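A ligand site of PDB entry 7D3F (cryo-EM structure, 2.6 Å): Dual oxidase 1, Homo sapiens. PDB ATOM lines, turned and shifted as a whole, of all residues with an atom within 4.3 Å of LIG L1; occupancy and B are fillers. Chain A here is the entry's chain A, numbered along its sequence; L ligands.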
ATOM      1  N   PHE A1097       6.945  -6.189   8.461  1.00  0.00           N
ATOM      2  CA  PHE A1097       8.212  -6.017   7.750  1.00  0.00           C
ATOM      3  C   PHE A1097       8.129  -6.551   6.330  1.00  0.00           C
ATOM      4  O   PHE A1097       8.815  -6.036   5.437  1.00  0.00           O
ATOM      5  CB  PHE A1097       9.353  -6.692   8.514  1.00  0.00           C
ATOM      6  CG  PHE A1097       9.869  -5.877   9.666  1.00  0.00           C
ATOM      7  CD1 PHE A1097      10.473  -4.660   9.459  1.00  0.00           C
ATOM      8  CD2 PHE A1097       9.763  -6.361  10.962  1.00  0.00           C
ATOM      9  CE1 PHE A1097      10.949  -3.922  10.520  1.00  0.00           C
ATOM     10  CE2 PHE A1097      10.254  -5.623  12.023  1.00  0.00           C
ATOM     11  CZ  PHE A1097      10.836  -4.402  11.805  1.00  0.00           C
ATOM     12  N   ILE A1100       5.738  -3.859   4.366  1.00  0.00           N
ATOM     13  CA  ILE A1100       6.186  -2.473   4.281  1.00  0.00           C
ATOM     14  C   ILE A1100       6.782  -2.175   2.904  1.00  0.00           C
ATOM     15  O   ILE A1100       6.891  -1.004   2.517  1.00  0.00           O
ATOM     16  CB  ILE A1100       7.196  -2.159   5.392  1.00  0.00           C
ATOM     17  CG1 ILE A1100       7.330  -0.647   5.595  1.00  0.00           C
ATOM     18  CG2 ILE A1100       8.551  -2.781   5.097  1.00  0.00           C
ATOM     19  CD1 ILE A1100       8.298  -0.259   6.690  1.00  0.00           C
ATOM     20  N   LEU A1101       7.175  -3.212   2.155  1.00  0.00           N
ATOM     21  CA  LEU A1101       7.728  -2.995   0.820  1.00  0.00           C
ATOM     22  C   LEU A1101       6.677  -2.484  -0.161  1.00  0.00           C
ATOM     23  O   LEU A1101       7.029  -1.797  -1.135  1.00  0.00           O
ATOM     24  CB  LEU A1101       8.351  -4.289   0.293  1.00  0.00           C
ATOM     25  CG  LEU A1101       9.530  -4.854   1.090  1.00  0.00           C
ATOM     26  CD1 LEU A1101       9.988  -6.174   0.494  1.00  0.00           C
ATOM     27  CD2 LEU A1101      10.683  -3.853   1.108  1.00  0.00           C
ATOM     28  N   MET A1104       6.607   1.197  -1.008  1.00  0.00           N
ATOM     29  CA  MET A1104       7.692   1.748  -1.821  1.00  0.00           C
ATOM     30  C   MET A1104       7.638   1.271  -3.265  1.00  0.00           C
ATOM     31  O   MET A1104       8.606   1.455  -4.007  1.00  0.00           O
ATOM     32  CB  MET A1104       9.038   1.418  -1.197  1.00  0.00           C
ATOM     33  CG  MET A1104       9.323   2.231   0.044  1.00  0.00           C
ATOM     34  SD  MET A1104       9.243   3.993  -0.317  1.00  0.00           S
ATOM     35  CE  MET A1104       8.867   4.672   1.297  1.00  0.00           C
ATOM     36  N   ARG A1106       6.867   2.322  -6.281  1.00  0.00           N
ATOM     37  CA  ARG A1106       6.546   3.606  -6.885  1.00  0.00           C
ATOM     38  C   ARG A1106       5.724   3.449  -8.158  1.00  0.00           C
ATOM     39  O   ARG A1106       4.750   4.182  -8.372  1.00  0.00           O
ATOM     40  CB  ARG A1106       7.827   4.385  -7.184  1.00  0.00           C
ATOM     41  CG  ARG A1106       8.101   5.547  -6.231  1.00  0.00           C
ATOM     42  CD  ARG A1106       8.739   5.073  -4.930  1.00  0.00           C
ATOM     43  NE  ARG A1106      10.091   4.586  -5.138  1.00  0.00           N
ATOM     44  CZ  ARG A1106      10.962   4.355  -4.156  1.00  0.00           C
ATOM     45  NH1 ARG A1106      10.617   4.581  -2.891  1.00  0.00           N
ATOM     46  NH2 ARG A1106      12.178   3.914  -4.435  1.00  0.00           N
ATOM     47  N   HIS A1130       4.325   4.336   5.108  1.00  0.00           N
ATOM     48  CA  HIS A1130       5.603   3.669   5.306  1.00  0.00           C
ATOM     49  C   HIS A1130       6.134   3.952   6.711  1.00  0.00           C
ATOM     50  O   HIS A1130       6.269   3.038   7.530  1.00  0.00           O
ATOM     51  CB  HIS A1130       6.593   4.115   4.241  1.00  0.00           C
ATOM     52  CG  HIS A1130       7.955   3.504   4.379  1.00  0.00           C
ATOM     53  ND1 HIS A1130       8.261   2.260   3.892  1.00  0.00           N
ATOM     54  CD2 HIS A1130       9.091   3.981   4.938  1.00  0.00           C
ATOM     55  CE1 HIS A1130       9.526   1.981   4.156  1.00  0.00           C
ATOM     56  NE2 HIS A1130      10.056   3.017   4.788  1.00  0.00           N
ATOM     57  N   ARG A1131       6.374   5.238   7.007  1.00  0.00           N
ATOM     58  CA  ARG A1131       6.889   5.603   8.320  1.00  0.00           C
ATOM     59  C   ARG A1131       6.004   5.021   9.416  1.00  0.00           C
ATOM     60  O   ARG A1131       6.500   4.387  10.351  1.00  0.00           O
ATOM     61  CB  ARG A1131       6.963   7.125   8.449  1.00  0.00           C
ATOM     62  CG  ARG A1131       8.012   7.786   7.568  1.00  0.00           C
ATOM     63  CD  ARG A1131       8.193   9.249   7.942  1.00  0.00           C
ATOM     64  NE  ARG A1131       9.201   9.911   7.131  1.00  0.00           N
ATOM     65  CZ  ARG A1131       8.934  10.603   6.032  1.00  0.00           C
ATOM     66  NH1 ARG A1131       7.683  10.732   5.606  1.00  0.00           N
ATOM     67  NH2 ARG A1131       9.924  11.179   5.343  1.00  0.00           N
ATOM     68  N   ALA A1134       6.695   1.433   9.954  1.00  0.00           N
ATOM     69  CA  ALA A1134       7.968   1.312  10.651  1.00  0.00           C
ATOM     70  C   ALA A1134       7.824   1.735  12.107  1.00  0.00           C
ATOM     71  O   ALA A1134       8.282   1.015  13.009  1.00  0.00           O
ATOM     72  CB  ALA A1134       9.039   2.152   9.954  1.00  0.00           C
ATOM     73  N   LEU A1202      18.333  -2.389  13.246  1.00  0.00           N
ATOM     74  CA  LEU A1202      17.125  -1.593  13.404  1.00  0.00           C
ATOM     75  C   LEU A1202      17.415  -0.281  14.120  1.00  0.00           C
ATOM     76  O   LEU A1202      16.886   0.769  13.742  1.00  0.00           O
ATOM     77  CB  LEU A1202      16.065  -2.381  14.175  1.00  0.00           C
ATOM     78  CG  LEU A1202      15.275  -3.422  13.401  1.00  0.00           C
ATOM     79  CD1 LEU A1202      14.249  -4.047  14.317  1.00  0.00           C
ATOM     80  CD2 LEU A1202      14.593  -2.789  12.206  1.00  0.00           C
ATOM     81  N   MET A1205      19.145   1.997  11.563  1.00  0.00           N
ATOM     82  CA  MET A1205      18.226   2.461  10.532  1.00  0.00           C
ATOM     83  C   MET A1205      17.239   3.486  11.082  1.00  0.00           C
ATOM     84  O   MET A1205      17.043   4.556  10.485  1.00  0.00           O
ATOM     85  CB  MET A1205      17.474   1.285   9.912  1.00  0.00           C
ATOM     86  CG  MET A1205      18.243   0.522   8.850  1.00  0.00           C
ATOM     87  SD  MET A1205      17.236  -0.719   8.019  1.00  0.00           S
ATOM     88  CE  MET A1205      15.893   0.301   7.402  1.00  0.00           C
ATOM     89  N   TYR A1206      16.628   3.193  12.221  1.00  0.00           N
ATOM     90  CA  TYR A1206      15.597   4.080  12.766  1.00  0.00           C
ATOM     91  C   TYR A1206      16.190   5.389  13.248  1.00  0.00           C
ATOM     92  O   TYR A1206      15.576   6.452  13.080  1.00  0.00           O
ATOM     93  CB  TYR A1206      14.839   3.373  13.892  1.00  0.00           C
ATOM     94  CG  TYR A1206      13.721   2.483  13.406  1.00  0.00           C
ATOM     95  CD1 TYR A1206      13.990   1.236  12.845  1.00  0.00           C
ATOM     96  CD2 TYR A1206      12.399   2.893  13.486  1.00  0.00           C
ATOM     97  CE1 TYR A1206      12.973   0.418  12.391  1.00  0.00           C
ATOM     98  CE2 TYR A1206      11.368   2.075  13.032  1.00  0.00           C
ATOM     99  CZ  TYR A1206      11.666   0.844  12.493  1.00  0.00           C
ATOM    100  OH  TYR A1206      10.650   0.034  12.033  1.00  0.00           O
ATOM    101  N   ALA A1209      17.277   7.322  10.000  1.00  0.00           N
ATOM    102  CA  ALA A1209      16.143   7.679   9.149  1.00  0.00           C
ATOM    103  C   ALA A1209      15.188   8.654   9.836  1.00  0.00           C
ATOM    104  O   ALA A1209      14.189   9.041   9.217  1.00  0.00           O
ATOM    105  CB  ALA A1209      15.369   6.429   8.720  1.00  0.00           C
ATOM    106  N   ARG A1214      17.683  13.100   9.190  1.00  0.00           N
ATOM    107  CA  ARG A1214      17.419  13.291   7.761  1.00  0.00           C
ATOM    108  C   ARG A1214      17.631  14.747   7.377  1.00  0.00           C
ATOM    109  O   ARG A1214      18.123  15.045   6.282  1.00  0.00           O
ATOM    110  CB  ARG A1214      16.007  12.826   7.413  1.00  0.00           C
ATOM    111  CG  ARG A1214      15.683  12.879   5.928  1.00  0.00           C
ATOM    112  CD  ARG A1214      14.431  12.080   5.608  1.00  0.00           C
ATOM    113  NE  ARG A1214      14.033  12.220   4.212  1.00  0.00           N
ATOM    114  CZ  ARG A1214      13.096  13.059   3.783  1.00  0.00           C
ATOM    115  NH1 ARG A1214      12.449  13.821   4.650  1.00  0.00           N
ATOM    116  NH2 ARG A1214      12.793  13.127   2.494  1.00  0.00           N
ATOM    117  N   PHE A1221      21.632   8.993   5.553  1.00  0.00           N
ATOM    118  CA  PHE A1221      20.281   8.440   5.584  1.00  0.00           C
ATOM    119  C   PHE A1221      20.163   7.243   4.648  1.00  0.00           C
ATOM    120  O   PHE A1221      19.724   6.162   5.064  1.00  0.00           O
ATOM    121  CB  PHE A1221      19.258   9.512   5.211  1.00  0.00           C
ATOM    122  CG  PHE A1221      17.895   8.968   4.873  1.00  0.00           C
ATOM    123  CD1 PHE A1221      17.004   8.643   5.883  1.00  0.00           C
ATOM    124  CD2 PHE A1221      17.516   8.785   3.556  1.00  0.00           C
ATOM    125  CE1 PHE A1221      15.748   8.134   5.576  1.00  0.00           C
ATOM    126  CE2 PHE A1221      16.261   8.285   3.243  1.00  0.00           C
ATOM    127  CZ  PHE A1221      15.384   7.959   4.253  1.00  0.00           C
ATOM    128  N   TRP A1222      20.577   7.412   3.388  1.00  0.00           N
ATOM    129  CA  TRP A1222      20.453   6.318   2.424  1.00  0.00           C
ATOM    130  C   TRP A1222      21.466   5.218   2.705  1.00  0.00           C
ATOM    131  O   TRP A1222      21.160   4.030   2.515  1.00  0.00           O
ATOM    132  CB  TRP A1222      20.590   6.847   1.000  1.00  0.00           C
ATOM    133  CG  TRP A1222      19.337   7.494   0.511  1.00  0.00           C
ATOM    134  CD1 TRP A1222      19.103   8.825   0.356  1.00  0.00           C
ATOM    135  CD2 TRP A1222      18.127   6.826   0.133  1.00  0.00           C
ATOM    136  NE1 TRP A1222      17.831   9.031  -0.116  1.00  0.00           N
ATOM    137  CE2 TRP A1222      17.208   7.827  -0.255  1.00  0.00           C
ATOM    138  CE3 TRP A1222      17.732   5.488   0.079  1.00  0.00           C
ATOM    139  CZ2 TRP A1222      15.916   7.520  -0.693  1.00  0.00           C
ATOM    140  CZ3 TRP A1222      16.461   5.192  -0.360  1.00  0.00           C
ATOM    141  CH2 TRP A1222      15.564   6.198  -0.744  1.00  0.00           C
ATOM    142  N   HIS A1225      19.800   3.323   5.336  1.00  0.00           N
ATOM    143  CA  HIS A1225      18.512   2.766   4.926  1.00  0.00           C
ATOM    144  C   HIS A1225      18.677   1.623   3.941  1.00  0.00           C
ATOM    145  O   HIS A1225      17.762   0.799   3.807  1.00  0.00           O
ATOM    146  CB  HIS A1225      17.644   3.866   4.311  1.00  0.00           C
ATOM    147  CG  HIS A1225      16.205   3.774   4.687  1.00  0.00           C
ATOM    148  ND1 HIS A1225      15.727   4.202   5.911  1.00  0.00           N
ATOM    149  CD2 HIS A1225      15.122   3.305   4.016  1.00  0.00           C
ATOM    150  CE1 HIS A1225      14.424   3.999   5.971  1.00  0.00           C
ATOM    151  NE2 HIS A1225      14.033   3.456   4.838  1.00  0.00           N
ATOM    152  N   HIS A1226      19.813   1.536   3.245  1.00  0.00           N
ATOM    153  CA  HIS A1226      20.059   0.395   2.384  1.00  0.00           C
ATOM    154  C   HIS A1226      20.372  -0.872   3.167  1.00  0.00           C
ATOM    155  O   HIS A1226      20.542  -1.939   2.552  1.00  0.00           O
ATOM    156  CB  HIS A1226      21.199   0.697   1.406  1.00  0.00           C
ATOM    157  CG  HIS A1226      20.776   1.539   0.244  1.00  0.00           C
ATOM    158  ND1 HIS A1226      19.739   1.187  -0.590  1.00  0.00           N
ATOM    159  CD2 HIS A1226      21.258   2.717  -0.225  1.00  0.00           C
ATOM    160  CE1 HIS A1226      19.593   2.115  -1.529  1.00  0.00           C
ATOM    161  NE2 HIS A1226      20.504   3.049  -1.325  1.00  0.00           N
ATOM    162  N   TYR A1228      18.299  -2.493   4.715  1.00  0.00           N
ATOM    163  CA  TYR A1228      17.114  -3.351   4.745  1.00  0.00           C
ATOM    164  C   TYR A1228      17.363  -4.679   4.034  1.00  0.00           C
ATOM    165  O   TYR A1228      16.716  -5.672   4.353  1.00  0.00           O
ATOM    166  CB  TYR A1228      15.908  -2.618   4.134  1.00  0.00           C
ATOM    167  CG  TYR A1228      15.902  -2.533   2.621  1.00  0.00           C
ATOM    168  CD1 TYR A1228      15.185  -3.452   1.862  1.00  0.00           C
ATOM    169  CD2 TYR A1228      16.595  -1.524   1.960  1.00  0.00           C
ATOM    170  CE1 TYR A1228      15.162  -3.370   0.482  1.00  0.00           C
ATOM    171  CE2 TYR A1228      16.579  -1.438   0.586  1.00  0.00           C
ATOM    172  CZ  TYR A1228      15.863  -2.366  -0.150  1.00  0.00           C
ATOM    173  OH  TYR A1228      15.847  -2.280  -1.524  1.00  0.00           O
ATOM    174  N   LEU A1231      18.775  -6.629   6.702  1.00  0.00           N
ATOM    175  CA  LEU A1231      17.692  -6.865   7.650  1.00  0.00           C
ATOM    176  C   LEU A1231      16.834  -8.041   7.207  1.00  0.00           C
ATOM    177  O   LEU A1231      16.501  -8.924   8.006  1.00  0.00           O
ATOM    178  CB  LEU A1231      16.851  -5.605   7.803  1.00  0.00           C
ATOM    179  CG  LEU A1231      15.732  -5.662   8.850  1.00  0.00           C
ATOM    180  CD1 LEU A1231      16.270  -5.334  10.232  1.00  0.00           C
ATOM    181  CD2 LEU A1231      14.586  -4.739   8.475  1.00  0.00           C
ATOM    182  N   TYR A1232      16.459  -8.077   5.925  1.00  0.00           N
ATOM    183  CA  TYR A1232      15.628  -9.163   5.435  1.00  0.00           C
ATOM    184  C   TYR A1232      16.394 -10.484   5.388  1.00  0.00           C
ATOM    185  O   TYR A1232      15.830 -11.542   5.664  1.00  0.00           O
ATOM    186  CB  TYR A1232      15.071  -8.821   4.050  1.00  0.00           C
ATOM    187  CG  TYR A1232      13.940  -7.809   4.096  1.00  0.00           C
ATOM    188  CD1 TYR A1232      12.809  -8.036   4.866  1.00  0.00           C
ATOM    189  CD2 TYR A1232      14.002  -6.632   3.353  1.00  0.00           C
ATOM    190  CE1 TYR A1232      11.775  -7.124   4.909  1.00  0.00           C
ATOM    191  CE2 TYR A1232      12.976  -5.708   3.395  1.00  0.00           C
ATOM    192  CZ  TYR A1232      11.866  -5.964   4.176  1.00  0.00           C
ATOM    193  OH  TYR A1232      10.833  -5.052   4.218  1.00  0.00           O
ATOM    194  N   TYR A1260       7.881  -5.775  -4.999  1.00  0.00           N
ATOM    195  CA  TYR A1260       8.848  -4.695  -4.866  1.00  0.00           C
ATOM    196  C   TYR A1260       9.980  -4.826  -5.885  1.00  0.00           C
ATOM    197  O   TYR A1260      10.406  -3.830  -6.474  1.00  0.00           O
ATOM    198  CB  TYR A1260       9.405  -4.665  -3.440  1.00  0.00           C
ATOM    199  CG  TYR A1260      10.515  -3.660  -3.225  1.00  0.00           C
ATOM    200  CD1 TYR A1260      10.235  -2.305  -3.067  1.00  0.00           C
ATOM    201  CD2 TYR A1260      11.842  -4.062  -3.171  1.00  0.00           C
ATOM    202  CE1 TYR A1260      11.237  -1.385  -2.866  1.00  0.00           C
ATOM    203  CE2 TYR A1260      12.858  -3.142  -2.971  1.00  0.00           C
ATOM    204  CZ  TYR A1260      12.556  -1.815  -2.818  1.00  0.00           C
ATOM    205  OH  TYR A1260      13.566  -0.899  -2.623  1.00  0.00           O
ATOM    206  N   LYS A1264      10.910  -2.226  -8.825  1.00  0.00           N
ATOM    207  CA  LYS A1264      12.264  -1.685  -8.960  1.00  0.00           C
ATOM    208  C   LYS A1264      12.809  -1.918 -10.359  1.00  0.00           C
ATOM    209  O   LYS A1264      13.453  -1.035 -10.938  1.00  0.00           O
ATOM    210  CB  LYS A1264      13.174  -2.309  -7.912  1.00  0.00           C
ATOM    211  CG  LYS A1264      14.204  -1.357  -7.336  1.00  0.00           C
ATOM    212  CD  LYS A1264      13.556  -0.403  -6.336  1.00  0.00           C
ATOM    213  CE  LYS A1264      14.497   0.730  -5.953  1.00  0.00           C
ATOM    214  NZ  LYS A1264      14.727   1.653  -7.096  1.00  0.00           N
ATOM    215  N   GLU A1317      17.717  11.229  -4.710  1.00  0.00           N
ATOM    216  CA  GLU A1317      16.331  10.957  -4.347  1.00  0.00           C
ATOM    217  C   GLU A1317      15.394  11.597  -5.354  1.00  0.00           C
ATOM    218  O   GLU A1317      15.561  12.768  -5.709  1.00  0.00           O
ATOM    219  CB  GLU A1317      16.059  11.488  -2.945  1.00  0.00           C
ATOM    220  CG  GLU A1317      14.942  10.775  -2.188  1.00  0.00           C
ATOM    221  CD  GLU A1317      14.797  11.271  -0.766  1.00  0.00           C
ATOM    222  OE1 GLU A1317      15.658  12.067  -0.324  1.00  0.00           O
ATOM    223  OE2 GLU A1317      13.831  10.870  -0.089  1.00  0.00           O
HETATM  224  C1  LIG L   1      12.499   4.250   1.552  1.00  0.00           C
HETATM  225  C2  LIG L   1      12.263  -0.008   3.881  1.00  0.00           C
HETATM  226  C3  LIG L   1      12.010   2.361   8.107  1.00  0.00           C
HETATM  227  C4  LIG L   1      11.465   6.539   5.712  1.00  0.00           C
HETATM  228  C5  LIG L   1      12.503   2.885   1.802  1.00  0.00           C
HETATM  229  C6  LIG L   1      12.669   1.824   0.829  1.00  0.00           C
HETATM  230  C7  LIG L   1      12.610   0.659   1.468  1.00  0.00           C
HETATM  231  C8  LIG L   1      12.392   0.928   2.880  1.00  0.00           C
HETATM  232  C9  LIG L   1      12.747  -0.741   0.830  1.00  0.00           C
HETATM  233  C10 LIG L   1      12.898   2.008  -0.686  1.00  0.00           C
HETATM  234  C11 LIG L   1      14.318   2.484  -0.951  1.00  0.00           C
HETATM  235  C12 LIG L   1      14.540   2.631  -2.431  1.00  0.00           C
HETATM  236  O1  LIG L   1      13.577   2.369  -3.209  1.00  0.00           O
HETATM  237  O2  LIG L   1      15.664   2.993  -2.836  1.00  0.00           O
HETATM  238  C13 LIG L   1      12.262   0.262   5.239  1.00  0.00           C
HETATM  239  C14 LIG L   1      12.454  -0.698   6.304  1.00  0.00           C
HETATM  240  C15 LIG L   1      12.374  -0.039   7.470  1.00  0.00           C
HETATM  241  C16 LIG L   1      12.150   1.365   7.175  1.00  0.00           C
HETATM  242  C17 LIG L   1      12.694  -2.212   6.061  1.00  0.00           C
HETATM  243  C18 LIG L   1      12.514  -0.551   8.931  1.00  0.00           C
HETATM  244  C19 LIG L   1      13.018  -1.735   9.257  1.00  0.00           C
HETATM  245  C20 LIG L   1      11.836   3.712   7.840  1.00  0.00           C
HETATM  246  C21 LIG L   1      11.727   4.772   8.829  1.00  0.00           C
HETATM  247  C22 LIG L   1      11.579   5.935   8.155  1.00  0.00           C
HETATM  248  C23 LIG L   1      11.592   5.624   6.739  1.00  0.00           C
HETATM  249  C24 LIG L   1      11.780   4.518  10.345  1.00  0.00           C
HETATM  250  C25 LIG L   1      11.405   7.382   8.703  1.00  0.00           C
HETATM  251  C26 LIG L   1      11.338   7.714   9.994  1.00  0.00           C
HETATM  252  C27 LIG L   1      11.757   6.294   4.384  1.00  0.00           C
HETATM  253  C28 LIG L   1      11.892   7.299   3.343  1.00  0.00           C
HETATM  254  C29 LIG L   1      12.172   6.678   2.194  1.00  0.00           C
HETATM  255  C30 LIG L   1      12.231   5.247   2.453  1.00  0.00           C
HETATM  256  C31 LIG L   1      11.728   8.824   3.532  1.00  0.00           C
HETATM  257  C32 LIG L   1      12.391   7.372   0.831  1.00  0.00           C
HETATM  258  C33 LIG L   1      11.299   6.969  -0.145  1.00  0.00           C
HETATM  259  C34 LIG L   1      11.520   7.656  -1.467  1.00  0.00           C
HETATM  260  O3  LIG L   1      12.462   8.492  -1.559  1.00  0.00           O
HETATM  261  O4  LIG L   1      10.763   7.374  -2.431  1.00  0.00           O
HETATM  262  N1  LIG L   1      12.331   2.300   3.042  1.00  0.00           N
HETATM  263  N2  LIG L   1      12.078   1.501   5.803  1.00  0.00           N
HETATM  264  N3  LIG L   1      11.760   4.271   6.585  1.00  0.00           N
HETATM  265  N4  LIG L   1      11.976   5.059   3.807  1.00  0.00           N
HETATM  266 FE1  LIG L   1      12.042   3.284   4.811  1.00  0.00          FE
HETATM  267  P1  LG2 L   2       9.434  15.395   3.766  1.00  0.00           P
HETATM  268  O1  LG2 L   2       9.757  14.057   3.162  1.00  0.00           O
HETATM  269  O2  LG2 L   2       9.719  15.645   5.231  1.00  0.00           O
HETATM  270  O3  LG2 L   2       7.867  15.683   3.553  1.00  0.00           O
HETATM  271  C1  LG2 L   2       6.898  14.947   4.293  1.00  0.00           C
HETATM  272  C2  LG2 L   2       5.651  14.762   3.438  1.00  0.00           C
HETATM  273  O4  LG2 L   2       6.029  14.720   2.051  1.00  0.00           O
HETATM  274  C3  LG2 L   2       4.964  13.456   3.763  1.00  0.00           C
HETATM  275  O5  LG2 L   2       3.576  13.687   4.040  1.00  0.00           O
HETATM  276  C4  LG2 L   2       5.110  12.592   2.531  1.00  0.00           C
HETATM  277  O6  LG2 L   2       3.860  11.973   2.206  1.00  0.00           O
HETATM  278  C5  LG2 L   2       5.532  13.540   1.422  1.00  0.00           C
HETATM  279  N1  LG2 L   2       6.615  12.923   0.616  1.00  0.00           N
HETATM  280  C6  LG2 L   2       7.942  12.978   0.902  1.00  0.00           C
HETATM  281  N2  LG2 L   2       8.666  12.317  -0.031  1.00  0.00           N
HETATM  282  C7  LG2 L   2       7.816  11.829  -0.940  1.00  0.00           C
HETATM  283  C8  LG2 L   2       7.920  11.038  -2.188  1.00  0.00           C
HETATM  284  N3  LG2 L   2       9.130  10.631  -2.662  1.00  0.00           N
HETATM  285  N4  LG2 L   2       6.776  10.737  -2.844  1.00  0.00           N
HETATM  286  C9  LG2 L   2       5.579  11.136  -2.399  1.00  0.00           C
HETATM  287  N5  LG2 L   2       5.407  11.867  -1.271  1.00  0.00           N
HETATM  288  C10 LG2 L   2       6.470  12.234  -0.519  1.00  0.00           C
HETATM  289  N6  LG2 L   2       4.894  19.418  -4.085  1.00  0.00           N
HETATM  290  C11 LG2 L   2       5.133  20.633  -4.638  1.00  0.00           C
HETATM  291  O7  LG2 L   2       5.642  21.518  -3.924  1.00  0.00           O
HETATM  292  N7  LG2 L   2       4.847  20.914  -5.921  1.00  0.00           N
HETATM  293  C12 LG2 L   2       4.291  20.021  -6.749  1.00  0.00           C
HETATM  294  O8  LG2 L   2       4.030  20.314  -7.930  1.00  0.00           O
HETATM  295  C13 LG2 L   2       3.993  18.668  -6.218  1.00  0.00           C
HETATM  296  N8  LG2 L   2       3.445  17.706  -6.988  1.00  0.00           N
HETATM  297  C14 LG2 L   2       3.183  16.480  -6.487  1.00  0.00           C
HETATM  298  C15 LG2 L   2       2.605  15.518  -7.308  1.00  0.00           C
HETATM  299  C16 LG2 L   2       2.335  14.255  -6.824  1.00  0.00           C
HETATM  300  C17 LG2 L   2       1.711  13.212  -7.725  1.00  0.00           C
HETATM  301  C18 LG2 L   2       2.645  13.920  -5.408  1.00  0.00           C
HETATM  302  C19 LG2 L   2       2.347  12.551  -4.865  1.00  0.00           C
HETATM  303  C20 LG2 L   2       3.209  14.882  -4.586  1.00  0.00           C
HETATM  304  C21 LG2 L   2       3.508  16.153  -5.060  1.00  0.00           C
HETATM  305  N9  LG2 L   2       4.094  17.143  -4.233  1.00  0.00           N
HETATM  306  C22 LG2 L   2       4.340  18.411  -4.797  1.00  0.00           C
HETATM  307  C23 LG2 L   2       4.434  16.914  -2.824  1.00  0.00           C
HETATM  308  C24 LG2 L   2       5.594  15.930  -2.639  1.00  0.00           C
HETATM  309  O9  LG2 L   2       5.301  15.086  -1.523  1.00  0.00           O
HETATM  310  C25 LG2 L   2       6.941  16.605  -2.427  1.00  0.00           C
HETATM  311  O10 LG2 L   2       7.932  15.936  -3.201  1.00  0.00           O
HETATM  312  C26 LG2 L   2       7.314  16.547  -0.949  1.00  0.00           C
HETATM  313  O11 LG2 L   2       6.693  17.636  -0.261  1.00  0.00           O
HETATM  314  C27 LG2 L   2       8.822  16.608  -0.727  1.00  0.00           C
HETATM  315  O12 LG2 L   2       9.036  16.446   0.675  1.00  0.00           O
HETATM  316  P2  LG2 L   2      10.501  16.424   1.354  1.00  0.00           P
HETATM  317  O13 LG2 L   2      11.126  15.069   1.122  1.00  0.00           O
HETATM  318  O14 LG2 L   2      11.262  17.660   0.946  1.00  0.00           O
HETATM  319  O15 LG2 L   2      10.087  16.589   2.899  1.00  0.00           O
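An iron atom (FE1) of LIG L1 is bound by a ring nitrogen (NE2) of His 1225 (2.0 Å).
A ring nitrogen (NE2) of His 1130 is bound to an iron atom (FE1) of LIG L1.
The guanidinium group (NH2) of Arg 1106 is in salt-bridge range of an oxygen (O1) of LIG L1 (2.4 Å).
An oxygen (O1) of LIG L1 sits at hydrogen-bond distance from the side-chain hydroxyl of Tyr 1260, at 3.3 Å.
O1 of LG2 L2 lies within salt-bridge range of NH2 of Arg 1131, at 3.6 Å.
O13 of LG2 L2 lies within salt-bridge range of NH2 of Arg 1214 (2.9 Å).
SD of Met 1104 is in hydrogen-bond range of NH1 of Arg 1106, 3.0 Å away.
The side-chain carboxylate (OE2) of Glu 1317 is in salt-bridge range of the guanidinium group (NH2) of Arg 1214.
OH of Tyr 1232 lies within hydrogen-bond range of O of Phe 1097.
The side-chain hydroxyl of Tyr 1228 sits at hydrogen-bond distance from the side-chain hydroxyl of Tyr 1260, at 2.9 Å.
The backbone carbonyl oxygen (O) of Ala 1134 sits at hydrogen-bond distance from the side-chain hydroxyl (OH) of Tyr 1206, at 2.7 Å.
O3 of LIG L1 lies close to OE2 of Glu 1317, 3.1 Å away.
Phe 1097 touches LIG L1 (CE1 to C19, 3.3 Å).
CD2 of Leu 1101 touches C9 of LIG L1 (3.7 Å).
CG of Met 1104 touches C6 of LIG L1, at 3.5 Å.
Arg 1131 touches LIG L1.
Ala 1134 touches LIG L1 (CB to C3, 3.5 Å).
Leu 1202 touches LIG L1 (CD2 to C19, 3.5 Å).
CE of Met 1205 touches C15 of LIG L1, 3.5 Å away.
CD2 of Tyr 1206 touches C24 of LIG L1, 3.6 Å away.
O of Ala 1209 touches C26 of LIG L1, at 3.2 Å.
Phe 1221 touches LIG L1 (CZ to C28, 3.7 Å).
CZ3 of Trp 1222 touches O2 of LIG L1, at 3.4 Å.
CE1 of Tyr 1228 touches C9 of LIG L1, 3.6 Å away.
Leu 1231 touches LIG L1 (CD2 to C19, 3.5 Å).
OH of Tyr 1232 touches C17 of LIG L1, 3.9 Å away.
Lys 1264 touches LIG L1 (CE to O1, 3.3 Å).
Hydrophobic or aromatic side chains within 4 Å of LIG L1: Phe 1097, Leu 1101, Met 1104, His 1130, Ala 1134, Leu 1202, Met 1205, Tyr 1206, Ala 1209, Phe 1221, Trp 1222, His 1225, Tyr 1228, Leu 1231 and Tyr 1260.
Of the 23 residues printed, 20 come within 4 Å of LIG L1.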
